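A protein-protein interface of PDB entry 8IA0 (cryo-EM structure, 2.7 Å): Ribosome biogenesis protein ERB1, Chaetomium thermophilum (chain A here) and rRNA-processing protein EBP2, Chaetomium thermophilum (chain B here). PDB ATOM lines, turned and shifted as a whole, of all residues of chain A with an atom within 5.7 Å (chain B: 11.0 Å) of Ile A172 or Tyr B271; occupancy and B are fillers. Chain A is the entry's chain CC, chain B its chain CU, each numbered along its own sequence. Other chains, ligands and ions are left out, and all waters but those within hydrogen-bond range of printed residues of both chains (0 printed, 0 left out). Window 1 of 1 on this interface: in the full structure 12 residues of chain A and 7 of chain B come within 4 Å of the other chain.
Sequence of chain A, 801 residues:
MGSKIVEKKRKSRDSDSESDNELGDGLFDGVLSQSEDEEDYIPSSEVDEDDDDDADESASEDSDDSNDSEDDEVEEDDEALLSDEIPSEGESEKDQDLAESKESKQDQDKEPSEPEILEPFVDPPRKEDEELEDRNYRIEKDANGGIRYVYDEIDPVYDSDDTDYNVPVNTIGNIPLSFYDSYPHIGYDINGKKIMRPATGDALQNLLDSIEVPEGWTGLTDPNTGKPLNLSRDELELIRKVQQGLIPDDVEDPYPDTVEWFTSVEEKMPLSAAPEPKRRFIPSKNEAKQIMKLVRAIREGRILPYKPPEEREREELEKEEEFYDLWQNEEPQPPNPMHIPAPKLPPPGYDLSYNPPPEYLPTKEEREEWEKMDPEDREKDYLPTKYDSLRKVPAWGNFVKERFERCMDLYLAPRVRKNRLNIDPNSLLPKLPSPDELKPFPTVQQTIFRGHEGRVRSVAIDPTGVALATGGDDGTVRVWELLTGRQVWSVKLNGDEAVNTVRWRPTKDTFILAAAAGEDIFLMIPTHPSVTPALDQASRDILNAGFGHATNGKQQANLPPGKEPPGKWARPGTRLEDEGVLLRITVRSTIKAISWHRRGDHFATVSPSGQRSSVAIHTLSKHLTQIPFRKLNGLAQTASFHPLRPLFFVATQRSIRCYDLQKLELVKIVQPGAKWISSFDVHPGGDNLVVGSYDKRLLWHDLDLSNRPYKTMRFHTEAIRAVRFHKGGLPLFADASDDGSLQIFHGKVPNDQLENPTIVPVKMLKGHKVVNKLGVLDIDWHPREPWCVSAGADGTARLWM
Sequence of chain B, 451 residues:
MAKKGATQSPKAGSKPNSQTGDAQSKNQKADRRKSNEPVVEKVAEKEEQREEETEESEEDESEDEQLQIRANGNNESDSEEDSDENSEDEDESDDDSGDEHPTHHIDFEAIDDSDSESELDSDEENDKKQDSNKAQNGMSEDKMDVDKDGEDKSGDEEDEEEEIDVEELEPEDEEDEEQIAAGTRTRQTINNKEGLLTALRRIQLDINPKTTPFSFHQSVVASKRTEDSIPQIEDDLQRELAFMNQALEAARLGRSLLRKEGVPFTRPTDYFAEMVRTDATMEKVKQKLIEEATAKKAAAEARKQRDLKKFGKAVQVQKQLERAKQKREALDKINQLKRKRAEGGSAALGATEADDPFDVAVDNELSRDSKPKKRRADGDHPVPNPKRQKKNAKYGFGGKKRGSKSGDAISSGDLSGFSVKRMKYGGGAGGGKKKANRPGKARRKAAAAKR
The guanidinium group of Arg B267 is in hydrogen-bond range of the backbone carbonyl oxygen of Tyr B271, at 2.9 Å. O of Asn A170 sits close to O of Tyr A188, 2.7 Å away. OG1 of Thr A171 lies close to O of Tyr A188 (3.3 Å).
Ile A172 touches just these residues of chain B: Tyr B271, Phe B272 and Ala B273. Printed residues of chain A within 4 Å of Tyr B271: Thr A171, Ile A172, Tyr A180 and Tyr A188. Gly A173 touches just one residue of chain B: Glu B274 (3.1 Å). Of chain B, only Phe B272, Ala B273 and Glu B274 come within 4 Å of Ile A175. No residue of chain B comes within 4 Å of Gly A187. Of the printed residues of chain B, Tyr A188 touches Pro B268, Asp B270 and Tyr B271. Printed residues of chain A within 4 Å of Ala B273: Ile A172 (3.8 Å) and Ile A175 (3.6 Å). Printed residues of chain B within 4 Å of Asn A174: Glu B274. Pro A168 touches none of the printed residues of chain B.
Of the 14 printed residues of chain A, 8 touch a printed residue of chain B. Hydrophobic or aromatic side chains of chain A that line the printed part of chain B: Ile A172, Ile A175, Tyr A180, His A185 and Tyr A188. Among the printed residues, no Asp or Glu carboxylate lies within 4 Å of a Lys or Arg side-chain nitrogen of the other chain.
OD1 of Asp B270 lies within hydrogen-bond range of OH of Tyr A188 (2.8 Å). The side-chain hydroxyl (OH) of Tyr B271 sits at hydrogen-bond distance from the backbone carbonyl oxygen (O) of Thr A171. The side-chain hydroxyl of Tyr A180 sits at hydrogen-bond distance from the backbone carbonyl oxygen of Phe B272. The side-chain carboxylate of Glu B274 is in hydrogen-bond range of the backbone NH of Asn A174, 2.6 Å away.
Tyr B271 touches Ile A172. CD1 of Ile A172 touches CB of Ala B273, at 3.8 Å. Gly A173 touches Glu B274 (CA to OE1, 3.1 Å). Phe B272 touches Ile A175 (O to CD1, 3.2 Å). Ile A175 touches Ala B273. Glu B274 touches Ile A175 (N to CG2, 3.4 Å). OH of Tyr A180 touches CD1 of Tyr B271 (3.5 Å). CE1 of His A185 touches O of Asp B270, 3.3 Å away. Tyr A188 touches Pro B268 (OH to CG, 3.7 Å). Tyr A188 touches Tyr B271.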
ATOM      1  N   PRO A 168      17.902  26.052 -24.257  1.00  0.00           N
ATOM      2  CA  PRO A 168      19.276  26.290 -23.803  1.00  0.00           C
ATOM      3  C   PRO A 168      20.285  26.166 -24.935  1.00  0.00           C
ATOM      4  O   PRO A 168      20.050  25.523 -25.959  1.00  0.00           O
ATOM      5  CB  PRO A 168      19.494  25.202 -22.747  1.00  0.00           C
ATOM      6  CG  PRO A 168      18.532  24.130 -23.111  1.00  0.00           C
ATOM      7  CD  PRO A 168      17.334  24.821 -23.683  1.00  0.00           C
ATOM      8  N   ASN A 170      23.221  24.788 -24.384  1.00  0.00           N
ATOM      9  CA  ASN A 170      24.149  23.718 -24.040  1.00  0.00           C
ATOM     10  C   ASN A 170      23.990  22.499 -24.940  1.00  0.00           C
ATOM     11  O   ASN A 170      24.933  21.711 -25.071  1.00  0.00           O
ATOM     12  CB  ASN A 170      23.970  23.316 -22.579  1.00  0.00           C
ATOM     13  CG  ASN A 170      25.126  22.487 -22.062  1.00  0.00           C
ATOM     14  OD1 ASN A 170      26.192  22.444 -22.670  1.00  0.00           O
ATOM     15  ND2 ASN A 170      24.922  21.826 -20.929  1.00  0.00           N
ATOM     16  N   THR A 171      22.815  22.314 -25.543  1.00  0.00           N
ATOM     17  CA  THR A 171      22.546  21.168 -26.417  1.00  0.00           C
ATOM     18  C   THR A 171      22.845  19.856 -25.688  1.00  0.00           C
ATOM     19  O   THR A 171      23.225  18.846 -26.283  1.00  0.00           O
ATOM     20  CB  THR A 171      23.336  21.278 -27.725  1.00  0.00           C
ATOM     21  OG1 THR A 171      23.238  22.616 -28.223  1.00  0.00           O
ATOM     22  CG2 THR A 171      22.773  20.348 -28.782  1.00  0.00           C
ATOM     23  N   ILE A 172      22.677  19.877 -24.373  1.00  0.00           N
ATOM     24  CA  ILE A 172      22.885  18.714 -23.524  1.00  0.00           C
ATOM     25  C   ILE A 172      21.544  18.360 -22.906  1.00  0.00           C
ATOM     26  O   ILE A 172      20.892  19.215 -22.297  1.00  0.00           O
ATOM     27  CB  ILE A 172      23.943  18.987 -22.438  1.00  0.00           C
ATOM     28  CG1 ILE A 172      25.338  19.043 -23.059  1.00  0.00           C
ATOM     29  CG2 ILE A 172      23.882  17.934 -21.349  1.00  0.00           C
ATOM     30  CD1 ILE A 172      25.603  17.936 -24.044  1.00  0.00           C
ATOM     31  N   GLY A 173      21.133  17.109 -23.067  1.00  0.00           N
ATOM     32  CA  GLY A 173      19.811  16.678 -22.655  1.00  0.00           C
ATOM     33  C   GLY A 173      19.664  16.531 -21.158  1.00  0.00           C
ATOM     34  O   GLY A 173      20.275  17.259 -20.368  1.00  0.00           O
ATOM     35  N   ASN A 174      18.839  15.566 -20.759  1.00  0.00           N
ATOM     36  CA  ASN A 174      18.517  15.321 -19.361  1.00  0.00           C
ATOM     37  C   ASN A 174      19.597  14.485 -18.667  1.00  0.00           C
ATOM     38  O   ASN A 174      19.412  14.052 -17.524  1.00  0.00           O
ATOM     39  CB  ASN A 174      17.124  14.669 -19.285  1.00  0.00           C
ATOM     40  CG  ASN A 174      16.768  14.147 -17.905  1.00  0.00           C
ATOM     41  OD1 ASN A 174      17.210  13.071 -17.505  1.00  0.00           O
ATOM     42  ND2 ASN A 174      15.980  14.918 -17.163  1.00  0.00           N
ATOM     43  N   ILE A 175      20.744  14.304 -19.312  1.00  0.00           N
ATOM     44  CA  ILE A 175      21.833  13.502 -18.763  1.00  0.00           C
ATOM     45  C   ILE A 175      22.422  14.195 -17.541  1.00  0.00           C
ATOM     46  O   ILE A 175      22.345  15.426 -17.425  1.00  0.00           O
ATOM     47  CB  ILE A 175      22.916  13.244 -19.821  1.00  0.00           C
ATOM     48  CG1 ILE A 175      23.662  14.540 -20.136  1.00  0.00           C
ATOM     49  CG2 ILE A 175      22.298  12.657 -21.071  1.00  0.00           C
ATOM     50  CD1 ILE A 175      25.089  14.338 -20.552  1.00  0.00           C
ATOM     51  N   LEU A 177      25.137  15.935 -15.076  1.00  0.00           N
ATOM     52  CA  LEU A 177      26.322  16.755 -15.274  1.00  0.00           C
ATOM     53  C   LEU A 177      27.562  16.159 -14.622  1.00  0.00           C
ATOM     54  O   LEU A 177      28.582  16.846 -14.522  1.00  0.00           O
ATOM     55  CB  LEU A 177      26.083  18.167 -14.738  1.00  0.00           C
ATOM     56  CG  LEU A 177      25.224  19.081 -15.610  1.00  0.00           C
ATOM     57  CD1 LEU A 177      25.071  20.447 -14.965  1.00  0.00           C
ATOM     58  CD2 LEU A 177      25.824  19.208 -16.996  1.00  0.00           C
ATOM     59  N   TYR A 180      31.626  15.574 -17.910  1.00  0.00           N
ATOM     60  CA  TYR A 180      32.268  16.880 -18.047  1.00  0.00           C
ATOM     61  C   TYR A 180      32.845  17.390 -16.734  1.00  0.00           C
ATOM     62  O   TYR A 180      33.325  18.527 -16.692  1.00  0.00           O
ATOM     63  CB  TYR A 180      31.335  17.967 -18.603  1.00  0.00           C
ATOM     64  CG  TYR A 180      30.646  17.637 -19.907  1.00  0.00           C
ATOM     65  CD1 TYR A 180      31.236  17.945 -21.120  1.00  0.00           C
ATOM     66  CD2 TYR A 180      29.394  17.046 -19.922  1.00  0.00           C
ATOM     67  CE1 TYR A 180      30.607  17.659 -22.310  1.00  0.00           C
ATOM     68  CE2 TYR A 180      28.760  16.755 -21.107  1.00  0.00           C
ATOM     69  CZ  TYR A 180      29.370  17.065 -22.297  1.00  0.00           C
ATOM     70  OH  TYR A 180      28.741  16.775 -23.483  1.00  0.00           O
ATOM     71  N   HIS A 185      35.573  21.924 -20.779  1.00  0.00           N
ATOM     72  CA  HIS A 185      34.364  22.376 -21.446  1.00  0.00           C
ATOM     73  C   HIS A 185      33.137  21.746 -20.804  1.00  0.00           C
ATOM     74  O   HIS A 185      33.222  20.743 -20.092  1.00  0.00           O
ATOM     75  CB  HIS A 185      34.405  22.031 -22.937  1.00  0.00           C
ATOM     76  CG  HIS A 185      34.332  20.565 -23.218  1.00  0.00           C
ATOM     77  ND1 HIS A 185      33.237  19.974 -23.811  1.00  0.00           N
ATOM     78  CD2 HIS A 185      35.216  19.567 -22.985  1.00  0.00           C
ATOM     79  CE1 HIS A 185      33.451  18.677 -23.932  1.00  0.00           C
ATOM     80  NE2 HIS A 185      34.643  18.404 -23.437  1.00  0.00           N
ATOM     81  N   ILE A 186      31.986  22.360 -21.062  1.00  0.00           N
ATOM     82  CA  ILE A 186      30.700  21.881 -20.555  1.00  0.00           C
ATOM     83  C   ILE A 186      29.731  21.880 -21.737  1.00  0.00           C
ATOM     84  O   ILE A 186      29.103  22.895 -22.056  1.00  0.00           O
ATOM     85  CB  ILE A 186      30.179  22.722 -19.384  1.00  0.00           C
ATOM     86  CG1 ILE A 186      28.774  22.281 -18.973  1.00  0.00           C
ATOM     87  CG2 ILE A 186      30.274  24.226 -19.668  1.00  0.00           C
ATOM     88  CD1 ILE A 186      28.741  20.922 -18.321  1.00  0.00           C
ATOM     89  N   GLY A 187      29.618  20.739 -22.408  1.00  0.00           N
ATOM     90  CA  GLY A 187      28.686  20.591 -23.507  1.00  0.00           C
ATOM     91  C   GLY A 187      29.207  21.116 -24.833  1.00  0.00           C
ATOM     92  O   GLY A 187      30.312  21.643 -24.955  1.00  0.00           O
ATOM     93  N   TYR A 188      28.363  20.962 -25.851  1.00  0.00           N
ATOM     94  CA  TYR A 188      28.630  21.415 -27.210  1.00  0.00           C
ATOM     95  C   TYR A 188      27.453  22.246 -27.690  1.00  0.00           C
ATOM     96  O   TYR A 188      26.309  21.959 -27.340  1.00  0.00           O
ATOM     97  CB  TYR A 188      28.825  20.234 -28.163  1.00  0.00           C
ATOM     98  CG  TYR A 188      30.238  19.725 -28.280  1.00  0.00           C
ATOM     99  CD1 TYR A 188      30.783  18.899 -27.308  1.00  0.00           C
ATOM    100  CD2 TYR A 188      31.021  20.056 -29.373  1.00  0.00           C
ATOM    101  CE1 TYR A 188      32.072  18.425 -27.419  1.00  0.00           C
ATOM    102  CE2 TYR A 188      32.308  19.588 -29.492  1.00  0.00           C
ATOM    103  CZ  TYR A 188      32.829  18.773 -28.513  1.00  0.00           C
ATOM    104  OH  TYR A 188      34.116  18.307 -28.633  1.00  0.00           O
ATOM    105  N   PRO A 223      23.289  23.862 -16.351  1.00  0.00           N
ATOM    106  CA  PRO A 223      23.943  23.119 -17.440  1.00  0.00           C
ATOM    107  C   PRO A 223      24.663  24.004 -18.441  1.00  0.00           C
ATOM    108  O   PRO A 223      25.692  23.588 -18.988  1.00  0.00           O
ATOM    109  CB  PRO A 223      22.780  22.359 -18.092  1.00  0.00           C
ATOM    110  CG  PRO A 223      21.554  23.103 -17.682  1.00  0.00           C
ATOM    111  CD  PRO A 223      21.838  23.623 -16.312  1.00  0.00           C
ATOM    112  N   PRO B 264      30.348  19.122 -39.390  1.00  0.00           N
ATOM    113  CA  PRO B 264      30.943  18.052 -38.583  1.00  0.00           C
ATOM    114  C   PRO B 264      30.097  16.789 -38.623  1.00  0.00           C
ATOM    115  O   PRO B 264      28.866  16.842 -38.618  1.00  0.00           O
ATOM    116  CB  PRO B 264      30.990  18.655 -37.176  1.00  0.00           C
ATOM    117  CG  PRO B 264      30.954  20.128 -37.395  1.00  0.00           C
ATOM    118  CD  PRO B 264      30.084  20.329 -38.592  1.00  0.00           C
ATOM    119  N   PHE B 265      30.774  15.642 -38.663  1.00  0.00           N
ATOM    120  CA  PHE B 265      30.109  14.354 -38.809  1.00  0.00           C
ATOM    121  C   PHE B 265      30.344  13.444 -37.611  1.00  0.00           C
ATOM    122  O   PHE B 265      29.378  12.946 -37.025  1.00  0.00           O
ATOM    123  CB  PHE B 265      30.580  13.680 -40.106  1.00  0.00           C
ATOM    124  CG  PHE B 265      29.713  12.539 -40.550  1.00  0.00           C
ATOM    125  CD1 PHE B 265      29.916  11.265 -40.055  1.00  0.00           C
ATOM    126  CD2 PHE B 265      28.702  12.739 -41.471  1.00  0.00           C
ATOM    127  CE1 PHE B 265      29.123  10.215 -40.461  1.00  0.00           C
ATOM    128  CE2 PHE B 265      27.906  11.694 -41.879  1.00  0.00           C
ATOM    129  CZ  PHE B 265      28.117  10.430 -41.375  1.00  0.00           C
ATOM    130  N   THR B 266      31.594  13.209 -37.228  1.00  0.00           N
ATOM    131  CA  THR B 266      31.904  12.245 -36.183  1.00  0.00           C
ATOM    132  C   THR B 266      31.585  12.812 -34.807  1.00  0.00           C
ATOM    133  O   THR B 266      31.860  13.979 -34.518  1.00  0.00           O
ATOM    134  CB  THR B 266      33.378  11.844 -36.248  1.00  0.00           C
ATOM    135  OG1 THR B 266      33.710  11.467 -37.591  1.00  0.00           O
ATOM    136  CG2 THR B 266      33.661  10.675 -35.318  1.00  0.00           C
ATOM    137  N   ARG B 267      31.004  11.974 -33.958  1.00  0.00           N
ATOM    138  CA  ARG B 267      30.711  12.367 -32.588  1.00  0.00           C
ATOM    139  C   ARG B 267      31.985  12.320 -31.757  1.00  0.00           C
ATOM    140  O   ARG B 267      32.608  11.257 -31.658  1.00  0.00           O
ATOM    141  CB  ARG B 267      29.659  11.448 -31.986  1.00  0.00           C
ATOM    142  CG  ARG B 267      29.060  11.949 -30.687  1.00  0.00           C
ATOM    143  CD  ARG B 267      28.430  10.813 -29.906  1.00  0.00           C
ATOM    144  NE  ARG B 267      27.829  11.280 -28.664  1.00  0.00           N
ATOM    145  CZ  ARG B 267      27.376  10.485 -27.706  1.00  0.00           C
ATOM    146  NH1 ARG B 267      27.430   9.170 -27.816  1.00  0.00           N
ATOM    147  NH2 ARG B 267      26.855  11.024 -26.608  1.00  0.00           N
ATOM    148  N   PRO B 268      32.410  13.428 -31.157  1.00  0.00           N
ATOM    149  CA  PRO B 268      33.619  13.403 -30.330  1.00  0.00           C
ATOM    150  C   PRO B 268      33.437  12.539 -29.094  1.00  0.00           C
ATOM    151  O   PRO B 268      32.337  12.405 -28.554  1.00  0.00           O
ATOM    152  CB  PRO B 268      33.823  14.874 -29.949  1.00  0.00           C
ATOM    153  CG  PRO B 268      33.002  15.647 -30.921  1.00  0.00           C
ATOM    154  CD  PRO B 268      31.840  14.777 -31.258  1.00  0.00           C
ATOM    155  N   THR B 269      34.547  11.951 -28.645  1.00  0.00           N
ATOM    156  CA  THR B 269      34.515  11.099 -27.463  1.00  0.00           C
ATOM    157  C   THR B 269      34.195  11.876 -26.195  1.00  0.00           C
ATOM    158  O   THR B 269      33.798  11.267 -25.195  1.00  0.00           O
ATOM    159  CB  THR B 269      35.852  10.377 -27.298  1.00  0.00           C
ATOM    160  OG1 THR B 269      36.914  11.338 -27.261  1.00  0.00           O
ATOM    161  CG2 THR B 269      36.082   9.421 -28.454  1.00  0.00           C
ATOM    162  N   ASP B 270      34.359  13.197 -26.207  1.00  0.00           N
ATOM    163  CA  ASP B 270      34.070  14.034 -25.053  1.00  0.00           C
ATOM    164  C   ASP B 270      32.689  14.676 -25.115  1.00  0.00           C
ATOM    165  O   ASP B 270      32.381  15.542 -24.289  1.00  0.00           O
ATOM    166  CB  ASP B 270      35.158  15.101 -24.890  1.00  0.00           C
ATOM    167  CG  ASP B 270      35.255  16.045 -26.080  1.00  0.00           C
ATOM    168  OD1 ASP B 270      34.322  16.100 -26.910  1.00  0.00           O
ATOM    169  OD2 ASP B 270      36.282  16.744 -26.186  1.00  0.00           O
ATOM    170  N   TYR B 271      31.855  14.281 -26.073  1.00  0.00           N
ATOM    171  CA  TYR B 271      30.497  14.803 -26.207  1.00  0.00           C
ATOM    172  C   TYR B 271      29.527  13.800 -25.595  1.00  0.00           C
ATOM    173  O   TYR B 271      29.138  12.824 -26.238  1.00  0.00           O
ATOM    174  CB  TYR B 271      30.158  15.078 -27.668  1.00  0.00           C
ATOM    175  CG  TYR B 271      28.770  15.642 -27.867  1.00  0.00           C
ATOM    176  CD1 TYR B 271      28.243  16.570 -26.980  1.00  0.00           C
ATOM    177  CD2 TYR B 271      27.985  15.245 -28.938  1.00  0.00           C
ATOM    178  CE1 TYR B 271      26.976  17.086 -27.157  1.00  0.00           C
ATOM    179  CE2 TYR B 271      26.717  15.756 -29.119  1.00  0.00           C
ATOM    180  CZ  TYR B 271      26.221  16.677 -28.226  1.00  0.00           C
ATOM    181  OH  TYR B 271      24.959  17.189 -28.403  1.00  0.00           O
ATOM    182  N   PHE B 272      29.135  14.047 -24.350  1.00  0.00           N
ATOM    183  CA  PHE B 272      28.139  13.238 -23.661  1.00  0.00           C
ATOM    184  C   PHE B 272      26.800  13.957 -23.733  1.00  0.00           C
ATOM    185  O   PHE B 272      26.679  15.091 -23.260  1.00  0.00           O
ATOM    186  CB  PHE B 272      28.537  12.993 -22.206  1.00  0.00           C
ATOM    187  CG  PHE B 272      29.995  12.709 -22.011  1.00  0.00           C
ATOM    188  CD1 PHE B 272      30.477  11.415 -22.086  1.00  0.00           C
ATOM    189  CD2 PHE B 272      30.884  13.733 -21.741  1.00  0.00           C
ATOM    190  CE1 PHE B 272      31.816  11.150 -21.904  1.00  0.00           C
ATOM    191  CE2 PHE B 272      32.224  13.473 -21.559  1.00  0.00           C
ATOM    192  CZ  PHE B 272      32.690  12.180 -21.641  1.00  0.00           C
ATOM    193  N   ALA B 273      25.801  13.302 -24.318  1.00  0.00           N
ATOM    194  CA  ALA B 273      24.484  13.905 -24.467  1.00  0.00           C
ATOM    195  C   ALA B 273      23.427  12.812 -24.438  1.00  0.00           C
ATOM    196  O   ALA B 273      23.736  11.619 -24.408  1.00  0.00           O
ATOM    197  CB  ALA B 273      24.391  14.729 -25.753  1.00  0.00           C
ATOM    198  N   GLU B 274      22.165  13.236 -24.447  1.00  0.00           N
ATOM    199  CA  GLU B 274      21.057  12.294 -24.394  1.00  0.00           C
ATOM    200  C   GLU B 274      20.952  11.483 -25.679  1.00  0.00           C
ATOM    201  O   GLU B 274      21.353  11.925 -26.759  1.00  0.00           O
ATOM    202  CB  GLU B 274      19.734  13.015 -24.144  1.00  0.00           C
ATOM    203  CG  GLU B 274      18.909  12.386 -23.033  1.00  0.00           C
ATOM    204  CD  GLU B 274      17.657  13.174 -22.701  1.00  0.00           C
ATOM    205  OE1 GLU B 274      17.692  14.418 -22.778  1.00  0.00           O
ATOM    206  OE2 GLU B 274      16.634  12.544 -22.363  1.00  0.00           O
ATOM    207  N   MET B 275      20.398  10.284 -25.548  1.00  0.00           N
ATOM    208  CA  MET B 275      20.183   9.372 -26.658  1.00  0.00           C
ATOM    209  C   MET B 275      18.693   9.095 -26.811  1.00  0.00           C
ATOM    210  O   MET B 275      17.866   9.540 -26.011  1.00  0.00           O
ATOM    211  CB  MET B 275      20.942   8.056 -26.447  1.00  0.00           C
ATOM    212  CG  MET B 275      22.415   8.213 -26.112  1.00  0.00           C
ATOM    213  SD  MET B 275      23.478   8.246 -27.564  1.00  0.00           S
ATOM    214  CE  MET B 275      23.803   9.996 -27.689  1.00  0.00           C
ATOM    215  N   ASP B 279      20.065   4.809 -20.756  1.00  0.00           N
ATOM    216  CA  ASP B 279      21.182   4.004 -20.272  1.00  0.00           C
ATOM    217  C   ASP B 279      20.702   2.653 -19.762  1.00  0.00           C
ATOM    218  O   ASP B 279      21.360   1.629 -19.979  1.00  0.00           O
ATOM    219  CB  ASP B 279      21.928   4.753 -19.168  1.00  0.00           C
ATOM    220  CG  ASP B 279      22.996   5.676 -19.710  1.00  0.00           C
ATOM    221  OD1 ASP B 279      22.998   5.926 -20.932  1.00  0.00           O
ATOM    222  OD2 ASP B 279      23.838   6.148 -18.916  1.00  0.00           O
